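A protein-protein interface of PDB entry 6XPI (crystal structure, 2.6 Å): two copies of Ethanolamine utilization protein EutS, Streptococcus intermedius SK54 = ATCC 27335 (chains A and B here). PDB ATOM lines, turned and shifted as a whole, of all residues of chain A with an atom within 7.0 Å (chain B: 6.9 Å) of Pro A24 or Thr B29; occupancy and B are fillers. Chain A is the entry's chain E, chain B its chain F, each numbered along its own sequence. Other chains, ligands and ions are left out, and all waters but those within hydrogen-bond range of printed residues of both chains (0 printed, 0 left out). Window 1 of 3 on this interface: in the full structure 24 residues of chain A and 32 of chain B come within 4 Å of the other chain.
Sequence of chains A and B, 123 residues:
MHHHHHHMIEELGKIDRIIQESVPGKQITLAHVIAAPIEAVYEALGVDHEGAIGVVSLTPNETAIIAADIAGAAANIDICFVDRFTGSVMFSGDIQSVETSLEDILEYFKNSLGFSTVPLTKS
The side-chain hydroxyl (OG1) of Thr A63 lies within hydrogen-bond range of the backbone carbonyl oxygen (O) of Pro A60 (2.7 Å).
NE2 of Gln B27 lies within hydrogen-bond range of OG1 of Thr B29, 2.8 Å away.
The backbone carbonyl oxygen (O) of Gln B27 sits at hydrogen-bond distance from the backbone NH (N) of Thr B59, 2.9 Å away.
The backbone carbonyl oxygen (O) of Ile B28 lies close to the backbone NH (N) of Val B118, 3.5 Å away.
O of Ser B57 lies within hydrogen-bond range of N of Thr B29, at 2.9 Å.
The backbone NH (N) of Ser B57 lies within hydrogen-bond range of the backbone carbonyl oxygen (O) of Leu B30 (3.0 Å).
2 positions are printed for both chains.
Of the 12 printed residues of chain A, 7 touch a printed residue of chain B.
Pro A24 touches just these residues of chain B: Gln B27, Thr B29 and Thr B59.
Thr B29 touches just these residues of chain A: Pro A24 (3.5 Å), Lys A26 (3.7 Å) and Pro A60 (3.9 Å).
Printed residues of chain B within 4 Å of Ser A22: Thr B59 (3.6 Å).
Of the printed residues of chain B, Pro A60 touches Thr B29 (3.9 Å) and Ser B57 (3.7 Å).
Of the printed residues of chain B, Glu A62 touches Leu B30 (3.9 Å) and Ser B57 (3.1 Å).
Of the printed residues of chain A, Thr B59 touches Ser A22 and Pro A24.
Ala B31 touches none of the printed residues of chain A.
The nearest residue of chain A that does not touch Thr B29 is Gly A25 (4.8 Å).
The side-chain carboxylate (OE1) of Glu A62 is in hydrogen-bond range of the side-chain hydroxyl (OG) of Ser B57, at 3.1 Å.
Among the printed residues, pairs that only touch across the chains: Ser A22 with Thr B59, Val A23 with Gln B27, Pro A24 with Gln B27, Pro A24 with Thr B29, Pro A24 with Thr B59, Lys A26 with Thr B29, Lys A26 with Val B118, Pro A60 with Thr B29, Pro A60 with Ser B57, Glu A62 with Leu B30 and Thr A63 with Leu B30.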
ATOM      1  N   SER A  22      19.700 -34.648  30.584  1.00  0.00           N
ATOM      2  CA  SER A  22      20.230 -33.945  29.443  1.00  0.00           C
ATOM      3  C   SER A  22      20.363 -32.444  29.643  1.00  0.00           C
ATOM      4  O   SER A  22      19.383 -31.750  29.906  1.00  0.00           O
ATOM      5  CB  SER A  22      19.381 -34.235  28.213  1.00  0.00           C
ATOM      6  OG  SER A  22      20.071 -33.859  27.031  1.00  0.00           O
ATOM      7  N   VAL A  23      21.584 -31.951  29.510  1.00  0.00           N
ATOM      8  CA  VAL A  23      21.938 -30.535  29.563  1.00  0.00           C
ATOM      9  C   VAL A  23      22.873 -30.273  28.390  1.00  0.00           C
ATOM     10  O   VAL A  23      23.519 -31.204  27.907  1.00  0.00           O
ATOM     11  CB  VAL A  23      22.611 -30.117  30.899  1.00  0.00           C
ATOM     12  CG1 VAL A  23      21.670 -30.299  32.088  1.00  0.00           C
ATOM     13  CG2 VAL A  23      23.933 -30.843  31.109  1.00  0.00           C
ATOM     14  N   PRO A  24      22.972 -29.029  27.892  1.00  0.00           N
ATOM     15  CA  PRO A  24      23.892 -28.777  26.764  1.00  0.00           C
ATOM     16  C   PRO A  24      25.337 -28.651  27.227  1.00  0.00           C
ATOM     17  O   PRO A  24      25.616 -28.093  28.288  1.00  0.00           O
ATOM     18  CB  PRO A  24      23.396 -27.455  26.192  1.00  0.00           C
ATOM     19  CG  PRO A  24      22.801 -26.760  27.366  1.00  0.00           C
ATOM     20  CD  PRO A  24      22.253 -27.809  28.294  1.00  0.00           C
ATOM     21  N   GLY A  25      26.244 -29.177  26.434  1.00  0.00           N
ATOM     22  CA  GLY A  25      27.669 -29.041  26.695  1.00  0.00           C
ATOM     23  C   GLY A  25      28.174 -27.696  26.201  1.00  0.00           C
ATOM     24  O   GLY A  25      27.441 -26.961  25.531  1.00  0.00           O
ATOM     25  N   LYS A  26      29.411 -27.337  26.543  1.00  0.00           N
ATOM     26  CA  LYS A  26      29.953 -26.044  26.142  1.00  0.00           C
ATOM     27  C   LYS A  26      31.048 -26.192  25.111  1.00  0.00           C
ATOM     28  O   LYS A  26      32.208 -26.374  25.488  1.00  0.00           O
ATOM     29  CB  LYS A  26      30.422 -25.250  27.374  1.00  0.00           C
ATOM     30  CG  LYS A  26      29.268 -24.700  28.181  1.00  0.00           C
ATOM     31  CD  LYS A  26      29.727 -24.045  29.466  1.00  0.00           C
ATOM     32  CE  LYS A  26      29.887 -25.053  30.571  1.00  0.00           C
ATOM     33  NZ  LYS A  26      28.607 -25.283  31.299  1.00  0.00           N
ATOM     34  N   GLN A  27      30.702 -26.106  23.814  1.00  0.00           N
ATOM     35  CA  GLN A  27      31.726 -26.268  22.780  1.00  0.00           C
ATOM     36  C   GLN A  27      31.415 -25.634  21.413  1.00  0.00           C
ATOM     37  O   GLN A  27      30.263 -25.456  21.024  1.00  0.00           O
ATOM     38  CB  GLN A  27      32.090 -27.766  22.596  1.00  0.00           C
ATOM     39  CG  GLN A  27      31.294 -28.546  21.562  1.00  0.00           C
ATOM     40  CD  GLN A  27      31.955 -29.859  21.205  1.00  0.00           C
ATOM     41  OE1 GLN A  27      32.757 -30.416  21.966  1.00  0.00           O
ATOM     42  NE2 GLN A  27      31.610 -30.395  20.037  1.00  0.00           N
ATOM     43  N   THR A  59      27.461 -24.624  20.977  1.00  0.00           N
ATOM     44  CA  THR A  59      26.587 -25.195  21.999  1.00  0.00           C
ATOM     45  C   THR A  59      27.019 -24.554  23.335  1.00  0.00           C
ATOM     46  O   THR A  59      28.216 -24.574  23.647  1.00  0.00           O
ATOM     47  CB  THR A  59      26.767 -26.723  22.095  1.00  0.00           C
ATOM     48  OG1 THR A  59      26.957 -27.302  20.804  1.00  0.00           O
ATOM     49  CG2 THR A  59      25.623 -27.397  22.816  1.00  0.00           C
ATOM     50  N   PRO A  60      26.099 -24.005  24.152  1.00  0.00           N
ATOM     51  CA  PRO A  60      24.653 -23.879  23.921  1.00  0.00           C
ATOM     52  C   PRO A  60      24.323 -22.930  22.775  1.00  0.00           C
ATOM     53  O   PRO A  60      25.130 -22.084  22.400  1.00  0.00           O
ATOM     54  CB  PRO A  60      24.122 -23.402  25.284  1.00  0.00           C
ATOM     55  CG  PRO A  60      25.276 -22.662  25.900  1.00  0.00           C
ATOM     56  CD  PRO A  60      26.509 -23.399  25.436  1.00  0.00           C
ATOM     57  N   ASN A  61      23.135 -23.097  22.192  1.00  0.00           N
ATOM     58  CA  ASN A  61      22.681 -22.322  21.044  1.00  0.00           C
ATOM     59  C   ASN A  61      22.627 -20.813  21.276  1.00  0.00           C
ATOM     60  O   ASN A  61      22.838 -20.062  20.333  1.00  0.00           O
ATOM     61  CB  ASN A  61      21.349 -22.865  20.562  1.00  0.00           C
ATOM     62  CG  ASN A  61      21.461 -24.272  20.003  1.00  0.00           C
ATOM     63  OD1 ASN A  61      22.563 -24.821  19.814  1.00  0.00           O
ATOM     64  ND2 ASN A  61      20.332 -24.889  19.686  1.00  0.00           N
ATOM     65  N   GLU A  62      22.414 -20.377  22.538  1.00  0.00           N
ATOM     66  CA  GLU A  62      22.373 -18.974  22.937  1.00  0.00           C
ATOM     67  C   GLU A  62      23.720 -18.270  22.717  1.00  0.00           C
ATOM     68  O   GLU A  62      23.738 -17.052  22.552  1.00  0.00           O
ATOM     69  CB  GLU A  62      21.984 -18.839  24.426  1.00  0.00           C
ATOM     70  CG  GLU A  62      20.571 -19.276  24.771  1.00  0.00           C
ATOM     71  CD  GLU A  62      20.335 -20.751  25.051  1.00  0.00           C
ATOM     72  OE1 GLU A  62      21.263 -21.560  24.838  1.00  0.00           O
ATOM     73  OE2 GLU A  62      19.215 -21.103  25.488  1.00  0.00           O
ATOM     74  N   THR A  63      24.843 -19.019  22.738  1.00  0.00           N
ATOM     75  CA  THR A  63      26.155 -18.414  22.541  1.00  0.00           C
ATOM     76  C   THR A  63      26.373 -17.881  21.121  1.00  0.00           C
ATOM     77  O   THR A  63      27.411 -17.250  20.875  1.00  0.00           O
ATOM     78  CB  THR A  63      27.303 -19.343  22.972  1.00  0.00           C
ATOM     79  OG1 THR A  63      27.352 -20.512  22.131  1.00  0.00           O
ATOM     80  CG2 THR A  63      27.226 -19.734  24.435  1.00  0.00           C
ATOM     81  N   PHE A 115      35.315 -23.161  26.986  1.00  0.00           N
ATOM     82  CA  PHE A 115      34.593 -24.027  26.071  1.00  0.00           C
ATOM     83  C   PHE A 115      35.593 -24.895  25.327  1.00  0.00           C
ATOM     84  O   PHE A 115      36.713 -24.465  25.060  1.00  0.00           O
ATOM     85  CB  PHE A 115      33.848 -23.184  25.023  1.00  0.00           C
ATOM     86  CG  PHE A 115      32.477 -22.679  25.387  1.00  0.00           C
ATOM     87  CD1 PHE A 115      32.227 -22.142  26.640  1.00  0.00           C
ATOM     88  CD2 PHE A 115      31.459 -22.666  24.452  1.00  0.00           C
ATOM     89  CE1 PHE A 115      30.972 -21.642  26.961  1.00  0.00           C
ATOM     90  CE2 PHE A 115      30.209 -22.160  24.772  1.00  0.00           C
ATOM     91  CZ  PHE A 115      29.968 -21.662  26.027  1.00  0.00           C
ATOM     92  N   GLN B  27      20.123 -27.051  35.128  1.00  0.00           N
ATOM     93  CA  GLN B  27      21.296 -26.181  35.098  1.00  0.00           C
ATOM     94  C   GLN B  27      21.178 -24.883  34.250  1.00  0.00           C
ATOM     95  O   GLN B  27      20.414 -24.795  33.291  1.00  0.00           O
ATOM     96  CB  GLN B  27      22.552 -26.974  34.675  1.00  0.00           C
ATOM     97  CG  GLN B  27      22.869 -27.013  33.175  1.00  0.00           C
ATOM     98  CD  GLN B  27      24.274 -27.501  32.906  1.00  0.00           C
ATOM     99  OE1 GLN B  27      24.861 -28.242  33.704  1.00  0.00           O
ATOM    100  NE2 GLN B  27      24.848 -27.113  31.771  1.00  0.00           N
ATOM    101  N   ILE B  28      21.969 -23.883  34.634  1.00  0.00           N
ATOM    102  CA  ILE B  28      22.133 -22.642  33.902  1.00  0.00           C
ATOM    103  C   ILE B  28      23.463 -22.842  33.214  1.00  0.00           C
ATOM    104  O   ILE B  28      24.472 -23.073  33.884  1.00  0.00           O
ATOM    105  CB  ILE B  28      22.146 -21.401  34.827  1.00  0.00           C
ATOM    106  CG1 ILE B  28      20.759 -21.173  35.440  1.00  0.00           C
ATOM    107  CG2 ILE B  28      22.640 -20.170  34.053  1.00  0.00           C
ATOM    108  CD1 ILE B  28      20.677 -20.023  36.369  1.00  0.00           C
ATOM    109  N   THR B  29      23.464 -22.838  31.886  1.00  0.00           N
ATOM    110  CA  THR B  29      24.675 -23.086  31.103  1.00  0.00           C
ATOM    111  C   THR B  29      25.384 -21.783  30.657  1.00  0.00           C
ATOM    112  O   THR B  29      26.575 -21.796  30.339  1.00  0.00           O
ATOM    113  CB  THR B  29      24.350 -24.010  29.934  1.00  0.00           C
ATOM    114  OG1 THR B  29      23.481 -25.065  30.368  1.00  0.00           O
ATOM    115  CG2 THR B  29      25.591 -24.614  29.303  1.00  0.00           C
ATOM    116  N   LEU B  30      24.664 -20.659  30.659  1.00  0.00           N
ATOM    117  CA  LEU B  30      25.217 -19.381  30.247  1.00  0.00           C
ATOM    118  C   LEU B  30      24.539 -18.236  31.023  1.00  0.00           C
ATOM    119  O   LEU B  30      23.311 -18.211  31.128  1.00  0.00           O
ATOM    120  CB  LEU B  30      25.008 -19.220  28.739  1.00  0.00           C
ATOM    121  CG  LEU B  30      25.485 -17.935  28.099  1.00  0.00           C
ATOM    122  CD1 LEU B  30      26.990 -17.906  28.008  1.00  0.00           C
ATOM    123  CD2 LEU B  30      24.920 -17.818  26.708  1.00  0.00           C
ATOM    124  N   ALA B  31      25.342 -17.333  31.614  1.00  0.00           N
ATOM    125  CA  ALA B  31      24.871 -16.156  32.334  1.00  0.00           C
ATOM    126  C   ALA B  31      25.860 -15.125  31.879  1.00  0.00           C
ATOM    127  O   ALA B  31      26.934 -15.005  32.462  1.00  0.00           O
ATOM    128  CB  ALA B  31      24.989 -16.368  33.837  1.00  0.00           C
ATOM    129  N   VAL B  56      20.855 -15.517  29.001  1.00  0.00           N
ATOM    130  CA  VAL B  56      20.778 -16.646  29.925  1.00  0.00           C
ATOM    131  C   VAL B  56      20.343 -17.923  29.202  1.00  0.00           C
ATOM    132  O   VAL B  56      19.412 -17.897  28.404  1.00  0.00           O
ATOM    133  CB  VAL B  56      19.832 -16.361  31.137  1.00  0.00           C
ATOM    134  CG1 VAL B  56      19.963 -17.441  32.215  1.00  0.00           C
ATOM    135  CG2 VAL B  56      20.060 -14.975  31.733  1.00  0.00           C
ATOM    136  N   SER B  57      20.993 -19.047  29.503  1.00  0.00           N
ATOM    137  CA  SER B  57      20.647 -20.350  28.929  1.00  0.00           C
ATOM    138  C   SER B  57      20.305 -21.242  30.095  1.00  0.00           C
ATOM    139  O   SER B  57      21.131 -21.402  30.988  1.00  0.00           O
ATOM    140  CB  SER B  57      21.838 -20.935  28.187  1.00  0.00           C
ATOM    141  OG  SER B  57      21.608 -22.281  27.802  1.00  0.00           O
ATOM    142  N   LEU B  58      19.088 -21.806  30.116  1.00  0.00           N
ATOM    143  CA  LEU B  58      18.627 -22.639  31.228  1.00  0.00           C
ATOM    144  C   LEU B  58      17.993 -23.955  30.783  1.00  0.00           C
ATOM    145  O   LEU B  58      17.406 -24.021  29.711  1.00  0.00           O
ATOM    146  CB  LEU B  58      17.587 -21.882  32.070  1.00  0.00           C
ATOM    147  CG  LEU B  58      17.815 -20.440  32.406  1.00  0.00           C
ATOM    148  CD1 LEU B  58      16.990 -19.558  31.503  1.00  0.00           C
ATOM    149  CD2 LEU B  58      17.400 -20.174  33.803  1.00  0.00           C
ATOM    150  N   THR B  59      18.019 -24.955  31.678  1.00  0.00           N
ATOM    151  CA  THR B  59      17.413 -26.276  31.528  1.00  0.00           C
ATOM    152  C   THR B  59      16.802 -26.639  32.891  1.00  0.00           C
ATOM    153  O   THR B  59      17.512 -26.558  33.893  1.00  0.00           O
ATOM    154  CB  THR B  59      18.467 -27.345  31.141  1.00  0.00           C
ATOM    155  OG1 THR B  59      19.421 -26.823  30.201  1.00  0.00           O
ATOM    156  CG2 THR B  59      17.831 -28.620  30.598  1.00  0.00           C
ATOM    157  N   SER B 116      22.747 -26.539  38.882  1.00  0.00           N
ATOM    158  CA  SER B 116      24.168 -26.344  38.601  1.00  0.00           C
ATOM    159  C   SER B 116      24.266 -25.004  37.876  1.00  0.00           C
ATOM    160  O   SER B 116      23.448 -24.727  37.009  1.00  0.00           O
ATOM    161  CB  SER B 116      24.697 -27.462  37.704  1.00  0.00           C
ATOM    162  OG  SER B 116      25.805 -28.117  38.300  1.00  0.00           O
ATOM    163  N   THR B 117      25.196 -24.141  38.269  1.00  0.00           N
ATOM    164  CA  THR B 117      25.304 -22.812  37.665  1.00  0.00           C
ATOM    165  C   THR B 117      26.697 -22.517  37.156  1.00  0.00           C
ATOM    166  O   THR B 117      27.676 -22.977  37.738  1.00  0.00           O
ATOM    167  CB  THR B 117      24.864 -21.718  38.663  1.00  0.00           C
ATOM    168  OG1 THR B 117      25.648 -21.814  39.852  1.00  0.00           O
ATOM    169  CG2 THR B 117      23.387 -21.784  39.003  1.00  0.00           C
ATOM    170  N   VAL B 118      26.795 -21.700  36.108  1.00  0.00           N
ATOM    171  CA  VAL B 118      28.079 -21.243  35.590  1.00  0.00           C
ATOM    172  C   VAL B 118      28.381 -19.837  36.181  1.00  0.00           C
ATOM    173  O   VAL B 118      27.487 -19.204  36.759  1.00  0.00           O
ATOM    174  CB  VAL B 118      28.038 -21.206  34.058  1.00  0.00           C
ATOM    175  CG1 VAL B 118      27.877 -22.607  33.494  1.00  0.00           C
ATOM    176  CG2 VAL B 118      26.927 -20.290  33.572  1.00  0.00           C
ATOM    177  N   PRO B 119      29.623 -19.316  36.067  1.00  0.00           N
ATOM    178  CA  PRO B 119      29.881 -17.955  36.569  1.00  0.00           C
ATOM    179  C   PRO B 119      29.342 -16.884  35.614  1.00  0.00           C
ATOM    180  O   PRO B 119      28.971 -17.181  34.476  1.00  0.00           O
ATOM    181  CB  PRO B 119      31.410 -17.890  36.674  1.00  0.00           C
ATOM    182  CG  PRO B 119      31.931 -19.179  36.099  1.00  0.00           C
ATOM    183  CD  PRO B 119      30.819 -19.885  35.416  1.00  0.00           C
